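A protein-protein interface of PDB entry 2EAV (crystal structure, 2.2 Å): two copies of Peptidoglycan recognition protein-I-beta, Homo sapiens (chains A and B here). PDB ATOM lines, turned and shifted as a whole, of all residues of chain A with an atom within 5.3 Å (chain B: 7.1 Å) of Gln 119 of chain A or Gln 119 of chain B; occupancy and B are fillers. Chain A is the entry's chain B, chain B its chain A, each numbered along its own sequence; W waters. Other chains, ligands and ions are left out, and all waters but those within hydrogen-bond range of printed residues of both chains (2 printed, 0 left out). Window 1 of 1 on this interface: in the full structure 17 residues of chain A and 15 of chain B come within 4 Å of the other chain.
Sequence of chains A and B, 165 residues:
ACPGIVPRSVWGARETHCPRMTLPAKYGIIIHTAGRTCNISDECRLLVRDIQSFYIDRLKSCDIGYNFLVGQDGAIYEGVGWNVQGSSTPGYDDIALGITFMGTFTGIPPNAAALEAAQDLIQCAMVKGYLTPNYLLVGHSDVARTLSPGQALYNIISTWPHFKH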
ATOM      1  N   LEU A 115      -4.534 -15.823   2.363  1.00  0.00           N
ATOM      2  CA  LEU A 115      -5.201 -15.448   3.605  1.00  0.00           C
ATOM      3  C   LEU A 115      -4.276 -15.586   4.807  1.00  0.00           C
ATOM      4  O   LEU A 115      -4.114 -14.649   5.587  1.00  0.00           O
ATOM      5  CB  LEU A 115      -6.457 -16.305   3.819  1.00  0.00           C
ATOM      6  CG  LEU A 115      -7.651 -16.031   2.894  1.00  0.00           C
ATOM      7  CD1 LEU A 115      -8.807 -16.972   3.251  1.00  0.00           C
ATOM      8  CD2 LEU A 115      -8.088 -14.562   3.018  1.00  0.00           C
ATOM      9  N   GLU A 116      -3.678 -16.762   4.953  1.00  0.00           N
ATOM     10  CA  GLU A 116      -2.767 -17.035   6.058  1.00  0.00           C
ATOM     11  C   GLU A 116      -1.687 -15.968   6.145  1.00  0.00           C
ATOM     12  O   GLU A 116      -1.440 -15.398   7.209  1.00  0.00           O
ATOM     13  CB  GLU A 116      -2.122 -18.418   5.878  1.00  0.00           C
ATOM     14  CG  GLU A 116      -0.982 -18.699   6.836  1.00  0.00           C
ATOM     15  CD  GLU A 116      -0.303 -20.016   6.549  1.00  0.00           C
ATOM     16  OE1 GLU A 116      -0.461 -20.524   5.408  1.00  0.00           O
ATOM     17  OE2 GLU A 116       0.396 -20.536   7.452  1.00  0.00           O
ATOM     18  N   ALA A 117      -1.057 -15.694   5.011  1.00  0.00           N
ATOM     19  CA  ALA A 117       0.004 -14.702   4.939  1.00  0.00           C
ATOM     20  C   ALA A 117      -0.435 -13.337   5.460  1.00  0.00           C
ATOM     21  O   ALA A 117       0.280 -12.697   6.240  1.00  0.00           O
ATOM     22  CB  ALA A 117       0.483 -14.571   3.517  1.00  0.00           C
ATOM     23  N   ALA A 118      -1.610 -12.891   5.027  1.00  0.00           N
ATOM     24  CA  ALA A 118      -2.106 -11.589   5.450  1.00  0.00           C
ATOM     25  C   ALA A 118      -2.151 -11.478   6.963  1.00  0.00           C
ATOM     26  O   ALA A 118      -1.709 -10.474   7.529  1.00  0.00           O
ATOM     27  CB  ALA A 118      -3.488 -11.333   4.859  1.00  0.00           C
ATOM     28  N   GLN A 119      -2.678 -12.508   7.621  1.00  0.00           N
ATOM     29  CA  GLN A 119      -2.772 -12.490   9.075  1.00  0.00           C
ATOM     30  C   GLN A 119      -1.424 -12.646   9.762  1.00  0.00           C
ATOM     31  O   GLN A 119      -1.186 -12.014  10.786  1.00  0.00           O
ATOM     32  CB  GLN A 119      -3.721 -13.579   9.581  1.00  0.00           C
ATOM     33  CG  GLN A 119      -5.168 -13.402   9.156  1.00  0.00           C
ATOM     34  CD  GLN A 119      -6.143 -13.759  10.267  1.00  0.00           C
ATOM     35  OE1 GLN A 119      -6.466 -12.920  11.109  1.00  0.00           O
ATOM     36  NE2 GLN A 119      -6.605 -15.014  10.282  1.00  0.00           N
ATOM     37  N   ASP A 120      -0.543 -13.482   9.214  1.00  0.00           N
ATOM     38  CA  ASP A 120       0.767 -13.660   9.835  1.00  0.00           C
ATOM     39  C   ASP A 120       1.471 -12.305   9.760  1.00  0.00           C
ATOM     40  O   ASP A 120       2.239 -11.933  10.647  1.00  0.00           O
ATOM     41  CB  ASP A 120       1.592 -14.741   9.120  1.00  0.00           C
ATOM     42  CG  ASP A 120       2.618 -15.396  10.042  1.00  0.00           C
ATOM     43  OD1 ASP A 120       3.556 -16.066   9.546  1.00  0.00           O
ATOM     44  OD2 ASP A 120       2.480 -15.245  11.277  1.00  0.00           O
ATOM     45  N   LEU A 121       1.184 -11.552   8.707  1.00  0.00           N
ATOM     46  CA  LEU A 121       1.768 -10.221   8.555  1.00  0.00           C
ATOM     47  C   LEU A 121       1.230  -9.278   9.643  1.00  0.00           C
ATOM     48  O   LEU A 121       1.985  -8.472  10.194  1.00  0.00           O
ATOM     49  CB  LEU A 121       1.435  -9.653   7.170  1.00  0.00           C
ATOM     50  CG  LEU A 121       1.953  -8.253   6.843  1.00  0.00           C
ATOM     51  CD1 LEU A 121       3.452  -8.184   7.080  1.00  0.00           C
ATOM     52  CD2 LEU A 121       1.627  -7.921   5.385  1.00  0.00           C
ATOM     53  N   ILE A 122      -0.070  -9.381   9.942  1.00  0.00           N
ATOM     54  CA  ILE A 122      -0.708  -8.539  10.957  1.00  0.00           C
ATOM     55  C   ILE A 122      -0.131  -8.905  12.323  1.00  0.00           C
ATOM     56  O   ILE A 122       0.184  -8.041  13.138  1.00  0.00           O
ATOM     57  CB  ILE A 122      -2.251  -8.763  11.020  1.00  0.00           C
ATOM     58  CG1 ILE A 122      -2.887  -8.575   9.635  1.00  0.00           C
ATOM     59  CG2 ILE A 122      -2.876  -7.825  12.025  1.00  0.00           C
ATOM     60  CD1 ILE A 122      -2.286  -7.475   8.840  1.00  0.00           C
ATOM     61  N   GLN A 123      -0.015 -10.204  12.563  1.00  0.00           N
ATOM     62  CA  GLN A 123       0.521 -10.709  13.810  1.00  0.00           C
ATOM     63  C   GLN A 123       1.943 -10.169  13.956  1.00  0.00           C
ATOM     64  O   GLN A 123       2.380  -9.819  15.060  1.00  0.00           O
ATOM     65  CB  GLN A 123       0.528 -12.236  13.775  1.00  0.00           C
ATOM     66  CG  GLN A 123       1.528 -12.897  14.719  1.00  0.00           C
ATOM     67  CD  GLN A 123       1.813 -14.335  14.338  1.00  0.00           C
ATOM     68  OE1 GLN A 123       0.901 -15.158  14.252  1.00  0.00           O
ATOM     69  NE2 GLN A 123       3.087 -14.645  14.100  1.00  0.00           N
ATOM     70  N   CYS A 124       2.658 -10.105  12.835  1.00  0.00           N
ATOM     71  CA  CYS A 124       4.022  -9.604  12.832  1.00  0.00           C
ATOM     72  C   CYS A 124       3.983  -8.158  13.317  1.00  0.00           C
ATOM     73  O   CYS A 124       4.601  -7.812  14.326  1.00  0.00           O
ATOM     74  CB  CYS A 124       4.610  -9.692  11.417  1.00  0.00           C
ATOM     75  SG  CYS A 124       6.290  -9.013  11.157  1.00  0.00           S
ATOM     76  N   THR A 159     -14.021 -11.727  10.259  1.00  0.00           N
ATOM     77  CA  THR A 159     -13.788 -12.754  11.271  1.00  0.00           C
ATOM     78  C   THR A 159     -12.371 -12.686  11.838  1.00  0.00           C
ATOM     79  O   THR A 159     -11.960 -13.575  12.591  1.00  0.00           O
ATOM     80  CB  THR A 159     -13.985 -14.171  10.705  1.00  0.00           C
ATOM     81  OG1 THR A 159     -12.847 -14.526   9.914  1.00  0.00           O
ATOM     82  CG2 THR A 159     -15.243 -14.234   9.845  1.00  0.00           C
ATOM     83  N   TRP A 160     -11.634 -11.635  11.476  1.00  0.00           N
ATOM     84  CA  TRP A 160     -10.260 -11.435  11.939  1.00  0.00           C
ATOM     85  C   TRP A 160     -10.197 -10.599  13.213  1.00  0.00           C
ATOM     86  O   TRP A 160     -11.062  -9.776  13.464  1.00  0.00           O
ATOM     87  CB  TRP A 160      -9.440 -10.739  10.851  1.00  0.00           C
ATOM     88  CG  TRP A 160      -9.200 -11.570   9.641  1.00  0.00           C
ATOM     89  CD1 TRP A 160      -9.753 -12.782   9.357  1.00  0.00           C
ATOM     90  CD2 TRP A 160      -8.317 -11.267   8.555  1.00  0.00           C
ATOM     91  NE1 TRP A 160      -9.268 -13.260   8.165  1.00  0.00           N
ATOM     92  CE2 TRP A 160      -8.384 -12.349   7.648  1.00  0.00           C
ATOM     93  CE3 TRP A 160      -7.474 -10.188   8.258  1.00  0.00           C
ATOM     94  CZ2 TRP A 160      -7.641 -12.383   6.468  1.00  0.00           C
ATOM     95  CZ3 TRP A 160      -6.733 -10.223   7.081  1.00  0.00           C
ATOM     96  CH2 TRP A 160      -6.823 -11.315   6.202  1.00  0.00           C
ATOM     97  N   PRO A 161      -9.155 -10.799  14.033  1.00  0.00           N
ATOM     98  CA  PRO A 161      -8.984 -10.054  15.286  1.00  0.00           C
ATOM     99  C   PRO A 161      -9.089  -8.540  15.099  1.00  0.00           C
ATOM    100  O   PRO A 161      -8.518  -7.970  14.161  1.00  0.00           O
ATOM    101  CB  PRO A 161      -7.588 -10.464  15.744  1.00  0.00           C
ATOM    102  CG  PRO A 161      -7.463 -11.846  15.232  1.00  0.00           C
ATOM    103  CD  PRO A 161      -8.054 -11.758  13.843  1.00  0.00           C
ATOM    104  N   PRO B   3      -7.998 -10.260  24.522  1.00  0.00           N
ATOM    105  CA  PRO B   3      -9.408 -10.278  24.921  1.00  0.00           C
ATOM    106  C   PRO B   3      -9.740 -10.466  26.396  1.00  0.00           C
ATOM    107  O   PRO B   3      -8.888 -10.821  27.215  1.00  0.00           O
ATOM    108  CB  PRO B   3      -9.976 -11.406  24.074  1.00  0.00           C
ATOM    109  CG  PRO B   3      -8.872 -12.379  24.086  1.00  0.00           C
ATOM    110  CD  PRO B   3      -7.657 -11.503  23.808  1.00  0.00           C
ATOM    111  N   VAL B  70     -15.022 -20.889  23.640  1.00  0.00           N
ATOM    112  CA  VAL B  70     -15.533 -19.694  22.977  1.00  0.00           C
ATOM    113  C   VAL B  70     -17.021 -19.825  22.701  1.00  0.00           C
ATOM    114  O   VAL B  70     -17.441 -20.634  21.876  1.00  0.00           O
ATOM    115  CB  VAL B  70     -14.806 -19.441  21.625  1.00  0.00           C
ATOM    116  CG1 VAL B  70     -15.193 -18.084  21.068  1.00  0.00           C
ATOM    117  CG2 VAL B  70     -13.309 -19.510  21.812  1.00  0.00           C
ATOM    118  N   ILE B  76     -14.849 -15.292  25.581  1.00  0.00           N
ATOM    119  CA  ILE B  76     -13.880 -16.348  25.849  1.00  0.00           C
ATOM    120  C   ILE B  76     -14.049 -16.733  27.307  1.00  0.00           C
ATOM    121  O   ILE B  76     -13.937 -15.882  28.197  1.00  0.00           O
ATOM    122  CB  ILE B  76     -12.427 -15.869  25.638  1.00  0.00           C
ATOM    123  CG1 ILE B  76     -12.231 -15.387  24.197  1.00  0.00           C
ATOM    124  CG2 ILE B  76     -11.471 -16.989  25.967  1.00  0.00           C
ATOM    125  CD1 ILE B  76     -12.879 -16.307  23.143  1.00  0.00           C
ATOM    126  N   ILE B  99      -8.267 -24.897  22.652  1.00  0.00           N
ATOM    127  CA  ILE B  99      -9.254 -23.845  22.508  1.00  0.00           C
ATOM    128  C   ILE B  99     -10.421 -24.411  21.745  1.00  0.00           C
ATOM    129  O   ILE B  99     -10.317 -24.731  20.549  1.00  0.00           O
ATOM    130  CB  ILE B  99      -8.689 -22.639  21.755  1.00  0.00           C
ATOM    131  CG1 ILE B  99      -7.401 -22.185  22.434  1.00  0.00           C
ATOM    132  CG2 ILE B  99      -9.726 -21.513  21.738  1.00  0.00           C
ATOM    133  CD1 ILE B  99      -6.880 -20.853  21.945  1.00  0.00           C
ATOM    134  N   PHE B 101     -14.625 -24.301  20.654  1.00  0.00           N
ATOM    135  CA  PHE B 101     -15.834 -23.541  20.437  1.00  0.00           C
ATOM    136  C   PHE B 101     -16.952 -24.404  20.983  1.00  0.00           C
ATOM    137  O   PHE B 101     -16.895 -25.631  20.884  1.00  0.00           O
ATOM    138  CB  PHE B 101     -16.041 -23.300  18.940  1.00  0.00           C
ATOM    139  CG  PHE B 101     -15.023 -22.377  18.329  1.00  0.00           C
ATOM    140  CD1 PHE B 101     -13.807 -22.866  17.866  1.00  0.00           C
ATOM    141  CD2 PHE B 101     -15.270 -21.009  18.249  1.00  0.00           C
ATOM    142  CE1 PHE B 101     -12.849 -22.006  17.332  1.00  0.00           C
ATOM    143  CE2 PHE B 101     -14.318 -20.137  17.717  1.00  0.00           C
ATOM    144  CZ  PHE B 101     -13.106 -20.636  17.259  1.00  0.00           C
ATOM    145  N   ALA B 114     -17.461 -15.153  17.432  1.00  0.00           N
ATOM    146  CA  ALA B 114     -16.694 -16.226  18.049  1.00  0.00           C
ATOM    147  C   ALA B 114     -15.315 -16.362  17.419  1.00  0.00           C
ATOM    148  O   ALA B 114     -14.297 -16.348  18.107  1.00  0.00           O
ATOM    149  CB  ALA B 114     -17.456 -17.541  17.937  1.00  0.00           C
ATOM    150  N   LEU B 115     -15.288 -16.495  16.101  1.00  0.00           N
ATOM    151  CA  LEU B 115     -14.038 -16.625  15.377  1.00  0.00           C
ATOM    152  C   LEU B 115     -13.071 -15.495  15.735  1.00  0.00           C
ATOM    153  O   LEU B 115     -11.896 -15.739  15.980  1.00  0.00           O
ATOM    154  CB  LEU B 115     -14.313 -16.624  13.872  1.00  0.00           C
ATOM    155  CG  LEU B 115     -15.267 -17.703  13.340  1.00  0.00           C
ATOM    156  CD1 LEU B 115     -15.562 -17.427  11.870  1.00  0.00           C
ATOM    157  CD2 LEU B 115     -14.645 -19.094  13.511  1.00  0.00           C
ATOM    158  N   GLU B 116     -13.564 -14.261  15.774  1.00  0.00           N
ATOM    159  CA  GLU B 116     -12.705 -13.125  16.087  1.00  0.00           C
ATOM    160  C   GLU B 116     -12.061 -13.278  17.467  1.00  0.00           C
ATOM    161  O   GLU B 116     -10.850 -13.095  17.623  1.00  0.00           O
ATOM    162  CB  GLU B 116     -13.504 -11.799  16.006  1.00  0.00           C
ATOM    163  CG  GLU B 116     -14.192 -11.582  14.632  1.00  0.00           C
ATOM    164  CD  GLU B 116     -14.886 -10.218  14.457  1.00  0.00           C
ATOM    165  OE1 GLU B 116     -14.187  -9.195  14.260  1.00  0.00           O
ATOM    166  OE2 GLU B 116     -16.141 -10.169  14.506  1.00  0.00           O
ATOM    167  N   ALA B 117     -12.873 -13.633  18.459  1.00  0.00           N
ATOM    168  CA  ALA B 117     -12.396 -13.782  19.825  1.00  0.00           C
ATOM    169  C   ALA B 117     -11.344 -14.870  19.994  1.00  0.00           C
ATOM    170  O   ALA B 117     -10.407 -14.714  20.767  1.00  0.00           O
ATOM    171  CB  ALA B 117     -13.571 -14.043  20.755  1.00  0.00           C
ATOM    172  N   ALA B 118     -11.506 -15.976  19.282  1.00  0.00           N
ATOM    173  CA  ALA B 118     -10.544 -17.065  19.381  1.00  0.00           C
ATOM    174  C   ALA B 118      -9.192 -16.600  18.858  1.00  0.00           C
ATOM    175  O   ALA B 118      -8.166 -16.782  19.517  1.00  0.00           O
ATOM    176  CB  ALA B 118     -11.023 -18.285  18.587  1.00  0.00           C
ATOM    177  N   GLN B 119      -9.193 -15.996  17.674  1.00  0.00           N
ATOM    178  CA  GLN B 119      -7.955 -15.522  17.070  1.00  0.00           C
ATOM    179  C   GLN B 119      -7.334 -14.419  17.900  1.00  0.00           C
ATOM    180  O   GLN B 119      -6.115 -14.354  18.058  1.00  0.00           O
ATOM    181  CB  GLN B 119      -8.212 -15.008  15.655  1.00  0.00           C
ATOM    182  CG  GLN B 119      -8.949 -15.989  14.786  1.00  0.00           C
ATOM    183  CD  GLN B 119      -8.622 -15.803  13.325  1.00  0.00           C
ATOM    184  OE1 GLN B 119      -7.514 -16.104  12.887  1.00  0.00           O
ATOM    185  NE2 GLN B 119      -9.583 -15.300  12.560  1.00  0.00           N
ATOM    186  N   ASP B 120      -8.175 -13.544  18.424  1.00  0.00           N
ATOM    187  CA  ASP B 120      -7.682 -12.447  19.239  1.00  0.00           C
ATOM    188  C   ASP B 120      -6.970 -13.101  20.417  1.00  0.00           C
ATOM    189  O   ASP B 120      -5.917 -12.650  20.858  1.00  0.00           O
ATOM    190  CB  ASP B 120      -8.857 -11.585  19.703  1.00  0.00           C
ATOM    191  CG  ASP B 120      -8.416 -10.263  20.286  1.00  0.00           C
ATOM    192  OD1 ASP B 120      -7.317  -9.797  19.930  1.00  0.00           O
ATOM    193  OD2 ASP B 120      -9.177  -9.676  21.081  1.00  0.00           O
ATOM    194  N   LEU B 121      -7.542 -14.197  20.899  1.00  0.00           N
ATOM    195  CA  LEU B 121      -6.955 -14.936  22.005  1.00  0.00           C
ATOM    196  C   LEU B 121      -5.659 -15.593  21.551  1.00  0.00           C
ATOM    197  O   LEU B 121      -4.673 -15.591  22.281  1.00  0.00           O
ATOM    198  CB  LEU B 121      -7.911 -16.019  22.499  1.00  0.00           C
ATOM    199  CG  LEU B 121      -7.391 -16.764  23.730  1.00  0.00           C
ATOM    200  CD1 LEU B 121      -7.458 -15.837  24.932  1.00  0.00           C
ATOM    201  CD2 LEU B 121      -8.227 -18.010  23.979  1.00  0.00           C
ATOM    202  N   ILE B 122      -5.666 -16.160  20.346  1.00  0.00           N
ATOM    203  CA  ILE B 122      -4.469 -16.816  19.824  1.00  0.00           C
ATOM    204  C   ILE B 122      -3.358 -15.784  19.688  1.00  0.00           C
ATOM    205  O   ILE B 122      -2.278 -15.928  20.270  1.00  0.00           O
ATOM    206  CB  ILE B 122      -4.696 -17.435  18.419  1.00  0.00           C
ATOM    207  CG1 ILE B 122      -5.870 -18.414  18.428  1.00  0.00           C
ATOM    208  CG2 ILE B 122      -3.437 -18.130  17.956  1.00  0.00           C
ATOM    209  CD1 ILE B 122      -5.709 -19.567  19.345  1.00  0.00           C
ATOM    210  N   GLN B 123      -3.626 -14.742  18.910  1.00  0.00           N
ATOM    211  CA  GLN B 123      -2.628 -13.705  18.692  1.00  0.00           C
ATOM    212  C   GLN B 123      -2.071 -13.219  20.030  1.00  0.00           C
ATOM    213  O   GLN B 123      -0.857 -13.103  20.188  1.00  0.00           O
ATOM    214  CB  GLN B 123      -3.224 -12.537  17.900  1.00  0.00           C
ATOM    215  CG  GLN B 123      -2.189 -11.504  17.469  1.00  0.00           C
ATOM    216  CD  GLN B 123      -2.756 -10.450  16.528  1.00  0.00           C
ATOM    217  OE1 GLN B 123      -3.580  -9.623  16.922  1.00  0.00           O
ATOM    218  NE2 GLN B 123      -2.319 -10.481  15.277  1.00  0.00           N
ATOM    219  N   CYS B 124      -2.955 -12.950  20.986  1.00  0.00           N
ATOM    220  CA  CYS B 124      -2.536 -12.485  22.308  1.00  0.00           C
ATOM    221  C   CYS B 124      -1.488 -13.408  22.901  1.00  0.00           C
ATOM    222  O   CYS B 124      -0.368 -12.993  23.209  1.00  0.00           O
ATOM    223  CB  CYS B 124      -3.709 -12.453  23.287  1.00  0.00           C
ATOM    224  SG  CYS B 124      -3.112 -12.140  24.980  1.00  0.00           S
ATOM    225  N   ALA B 125      -1.886 -14.665  23.076  1.00  0.00           N
ATOM    226  CA  ALA B 125      -1.031 -15.697  23.649  1.00  0.00           C
ATOM    227  C   ALA B 125       0.367 -15.713  23.051  1.00  0.00           C
ATOM    228  O   ALA B 125       1.352 -15.816  23.780  1.00  0.00           O
ATOM    229  CB  ALA B 125      -1.687 -17.069  23.482  1.00  0.00           C
ATOM    230  N   TYR B 135       4.555 -21.075  17.011  1.00  0.00           N
ATOM    231  CA  TYR B 135       3.606 -22.083  17.430  1.00  0.00           C
ATOM    232  C   TYR B 135       2.918 -22.744  16.240  1.00  0.00           C
ATOM    233  O   TYR B 135       2.772 -22.147  15.174  1.00  0.00           O
ATOM    234  CB  TYR B 135       2.561 -21.452  18.330  1.00  0.00           C
ATOM    235  CG  TYR B 135       1.638 -20.480  17.636  1.00  0.00           C
ATOM    236  CD1 TYR B 135       0.525 -20.928  16.922  1.00  0.00           C
ATOM    237  CD2 TYR B 135       1.851 -19.103  17.734  1.00  0.00           C
ATOM    238  CE1 TYR B 135      -0.358 -20.025  16.329  1.00  0.00           C
ATOM    239  CE2 TYR B 135       0.984 -18.198  17.155  1.00  0.00           C
ATOM    240  CZ  TYR B 135      -0.121 -18.663  16.455  1.00  0.00           C
ATOM    241  OH  TYR B 135      -0.987 -17.755  15.909  1.00  0.00           O
ATOM    242  N   LEU B 137      -0.503 -24.443  14.724  1.00  0.00           N
ATOM    243  CA  LEU B 137      -1.945 -24.379  14.892  1.00  0.00           C
ATOM    244  C   LEU B 137      -2.488 -25.630  14.247  1.00  0.00           C
ATOM    245  O   LEU B 137      -2.074 -25.990  13.143  1.00  0.00           O
ATOM    246  CB  LEU B 137      -2.539 -23.166  14.184  1.00  0.00           C
ATOM    247  CG  LEU B 137      -4.061 -23.111  14.376  1.00  0.00           C
ATOM    248  CD1 LEU B 137      -4.391 -22.642  15.795  1.00  0.00           C
ATOM    249  CD2 LEU B 137      -4.671 -22.183  13.365  1.00  0.00           C
ATOM    250  N   ILE B 156     -12.100 -23.113   7.984  1.00  0.00           N
ATOM    251  CA  ILE B 156     -11.666 -21.780   8.380  1.00  0.00           C
ATOM    252  C   ILE B 156     -10.276 -21.745   9.001  1.00  0.00           C
ATOM    253  O   ILE B 156      -9.408 -21.001   8.549  1.00  0.00           O
ATOM    254  CB  ILE B 156     -12.661 -21.133   9.390  1.00  0.00           C
ATOM    255  CG1 ILE B 156     -13.919 -20.657   8.664  1.00  0.00           C
ATOM    256  CG2 ILE B 156     -12.011 -19.945  10.088  1.00  0.00           C
ATOM    257  CD1 ILE B 156     -14.641 -21.744   7.905  1.00  0.00           C
ATOM    258  N   ILE B 157     -10.052 -22.541  10.038  1.00  0.00           N
ATOM    259  CA  ILE B 157      -8.752 -22.506  10.688  1.00  0.00           C
ATOM    260  C   ILE B 157      -7.594 -22.981   9.804  1.00  0.00           C
ATOM    261  O   ILE B 157      -6.427 -22.726  10.114  1.00  0.00           O
ATOM    262  CB  ILE B 157      -8.761 -23.302  12.024  1.00  0.00           C
ATOM    263  CG1 ILE B 157      -8.802 -24.804  11.762  1.00  0.00           C
ATOM    264  CG2 ILE B 157      -9.960 -22.874  12.868  1.00  0.00           C
ATOM    265  CD1 ILE B 157      -8.551 -25.618  13.001  1.00  0.00           C
ATOM    266  N   THR B 159      -6.870 -21.766   7.238  1.00  0.00           N
ATOM    267  CA  THR B 159      -6.459 -20.576   6.508  1.00  0.00           C
ATOM    268  C   THR B 159      -5.821 -19.641   7.515  1.00  0.00           C
ATOM    269  O   THR B 159      -5.339 -18.562   7.162  1.00  0.00           O
ATOM    270  CB  THR B 159      -7.631 -19.834   5.859  1.00  0.00           C
ATOM    271  OG1 THR B 159      -8.428 -19.227   6.879  1.00  0.00           O
ATOM    272  CG2 THR B 159      -8.473 -20.775   5.031  1.00  0.00           C
ATOM    273  N   TRP B 160      -5.817 -20.066   8.777  1.00  0.00           N
ATOM    274  CA  TRP B 160      -5.227 -19.271   9.850  1.00  0.00           C
ATOM    275  C   TRP B 160      -3.704 -19.388   9.858  1.00  0.00           C
ATOM    276  O   TRP B 160      -3.127 -20.291   9.245  1.00  0.00           O
ATOM    277  CB  TRP B 160      -5.776 -19.711  11.207  1.00  0.00           C
ATOM    278  CG  TRP B 160      -7.182 -19.292  11.459  1.00  0.00           C
ATOM    279  CD1 TRP B 160      -8.025 -18.658  10.584  1.00  0.00           C
ATOM    280  CD2 TRP B 160      -7.918 -19.467  12.672  1.00  0.00           C
ATOM    281  NE1 TRP B 160      -9.241 -18.427  11.183  1.00  0.00           N
ATOM    282  CE2 TRP B 160      -9.204 -18.914  12.465  1.00  0.00           C
ATOM    283  CE3 TRP B 160      -7.619 -20.041  13.918  1.00  0.00           C
ATOM    284  CZ2 TRP B 160     -10.190 -18.915  13.460  1.00  0.00           C
ATOM    285  CZ3 TRP B 160      -8.598 -20.046  14.904  1.00  0.00           C
ATOM    286  CH2 TRP B 160      -9.872 -19.485  14.669  1.00  0.00           C
ATOM    287  N   PRO B 161      -3.036 -18.461  10.563  1.00  0.00           N
ATOM    288  CA  PRO B 161      -1.574 -18.414  10.687  1.00  0.00           C
ATOM    289  C   PRO B 161      -0.967 -19.608  11.437  1.00  0.00           C
ATOM    290  O   PRO B 161      -1.512 -20.059  12.439  1.00  0.00           O
ATOM    291  CB  PRO B 161      -1.339 -17.095  11.430  1.00  0.00           C
ATOM    292  CG  PRO B 161      -2.531 -16.264  11.048  1.00  0.00           C
ATOM    293  CD  PRO B 161      -3.648 -17.252  11.140  1.00  0.00           C
HETATM  294  O   HOH W   1      -3.131 -11.574  13.074  1.00  0.00           O
HETATM  295  O   HOH W   2      -5.050 -13.862  13.377  1.00  0.00           O
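Water W1 lies within hydrogen-bond range of the side-chain amide nitrogen of Gln 123 of chain B, the backbone carbonyl oxygen of Gln 119 of chain A and the backbone NH of Gln 123 of chain A. Water W2 lies within hydrogen-bond range of the side-chain amide oxygen of Gln 119 of chain A and the side-chain amide oxygen of Gln 119 of chain B.
Among the printed residues, merely in contact across the chains: Gln 123 of chain A with Gln 123 of chain B (3.2 Å), Pro 161 of chain A with Gln 119 of chain B (3.3 Å), Gln 119 of chain A with Pro 161 of chain B (3.3 Å), Thr 159 of chain A with Glu 116 of chain B (3.5 Å), Glu 116 of chain A with Trp 160 of chain B (3.6 Å), Gln 123 of chain A with Tyr 135 of chain B (3.6 Å), Pro 161 of chain A with Asp 120 of chain B (3.7 Å), Thr 159 of chain A with Leu 115 of chain B (3.8 Å), Asp 120 of chain A with Pro 161 of chain B (3.9 Å), Glu 116 of chain A with Pro 161 of chain B (3.9 Å), Gln 119 of chain A with Trp 160 of chain B (3.9 Å), Leu 115 of chain A with Thr 159 of chain B (3.9 Å), Trp 160 of chain A with Gln 119 of chain B (3.97 Å) and Ile 122 of chain A with Gln 123 of chain B (3.9997 Å).
OE1 of Gln 119 of chain B is in hydrogen-bond range of NE2 of Gln 119 of chain A (3.0 Å). O of Thr 159 of chain A sits at hydrogen-bond distance from NE2 of Gln 119 of chain B. O of Thr 159 of chain B sits close to N of Glu 116 of chain A (3.3 Å). The backbone carbonyl oxygen of Trp 160 of chain A lies close to the side-chain carboxylate of Glu 116 of chain B (3.3 Å).
Of the 24 printed residues of chain B, 9 touch a printed residue of chain A. Hydrophobic or aromatic side chains of chain B that line the printed part of chain A: Leu 115, Tyr 135, Trp 160 and Pro 161. Hydrophobic or aromatic side chains of chain A within 4 Å of the printed part of chain B: Pro 161. Among the printed residues, no Asp or Glu carboxylate lies within 4 Å of a Lys or Arg side-chain nitrogen of the other chain.
OE1 of Gln 119 of chain B lies close to NE1 of Trp 160 of chain B, at 3.4 Å. O of Ile 156 of chain B lies within hydrogen-bond range of OG1 of Thr 159 of chain B, 2.6 Å away.
Of chain B, only Gln 119 (3.0 Å), Trp 160 (3.9 Å) and Pro 161 (3.3 Å) come within 4 Å of Gln 119 of chain A. Cys 124 of chain A touches none of the printed residues of chain B. Of the printed residues of chain B, Thr 159 of chain A touches Leu 115 (3.8 Å), Glu 116 (3.5 Å) and Gln 119 (2.9 Å). Phe 101 of chain B touches none of the printed residues of chain A. Of the printed residues of chain A, Leu 115 of chain B touches Thr 159. Of chain A, only Gln 119, Thr 159, Trp 160 and Pro 161 come within 4 Å of Gln 119 of chain B. Printed residues of chain A within 4 Å of Trp 160 of chain B: Glu 116 and Gln 119. Of the printed residues of chain A, Pro 161 of chain B touches Glu 116 (3.9 Å), Gln 119 (3.3 Å) and Asp 120 (3.9 Å). The nearest printed residue of chain A that does not touch Gln 119 of chain B is Gln 123 of chain A (8.0 Å).
Leu 115 of chain A touches Thr 159 of chain B, and with the chains exchanged Thr 159 of chain A touches Leu 115 of chain B. Glu 116 of chain A touches Pro 161 of chain B, but with the chains exchanged Pro 161 of chain A does not touch Glu 116 of chain B (4.3 Å). Gln 119 of chain B touches its own counterpart, Gln 119 of chain A. Gln 123 of chain A touches its own counterpart, Gln 123 of chain B. Positions printed for both chains: 115, 116, 117, 118, 119, 120, 121, 122, 123, 124, 159, 160 and 161.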
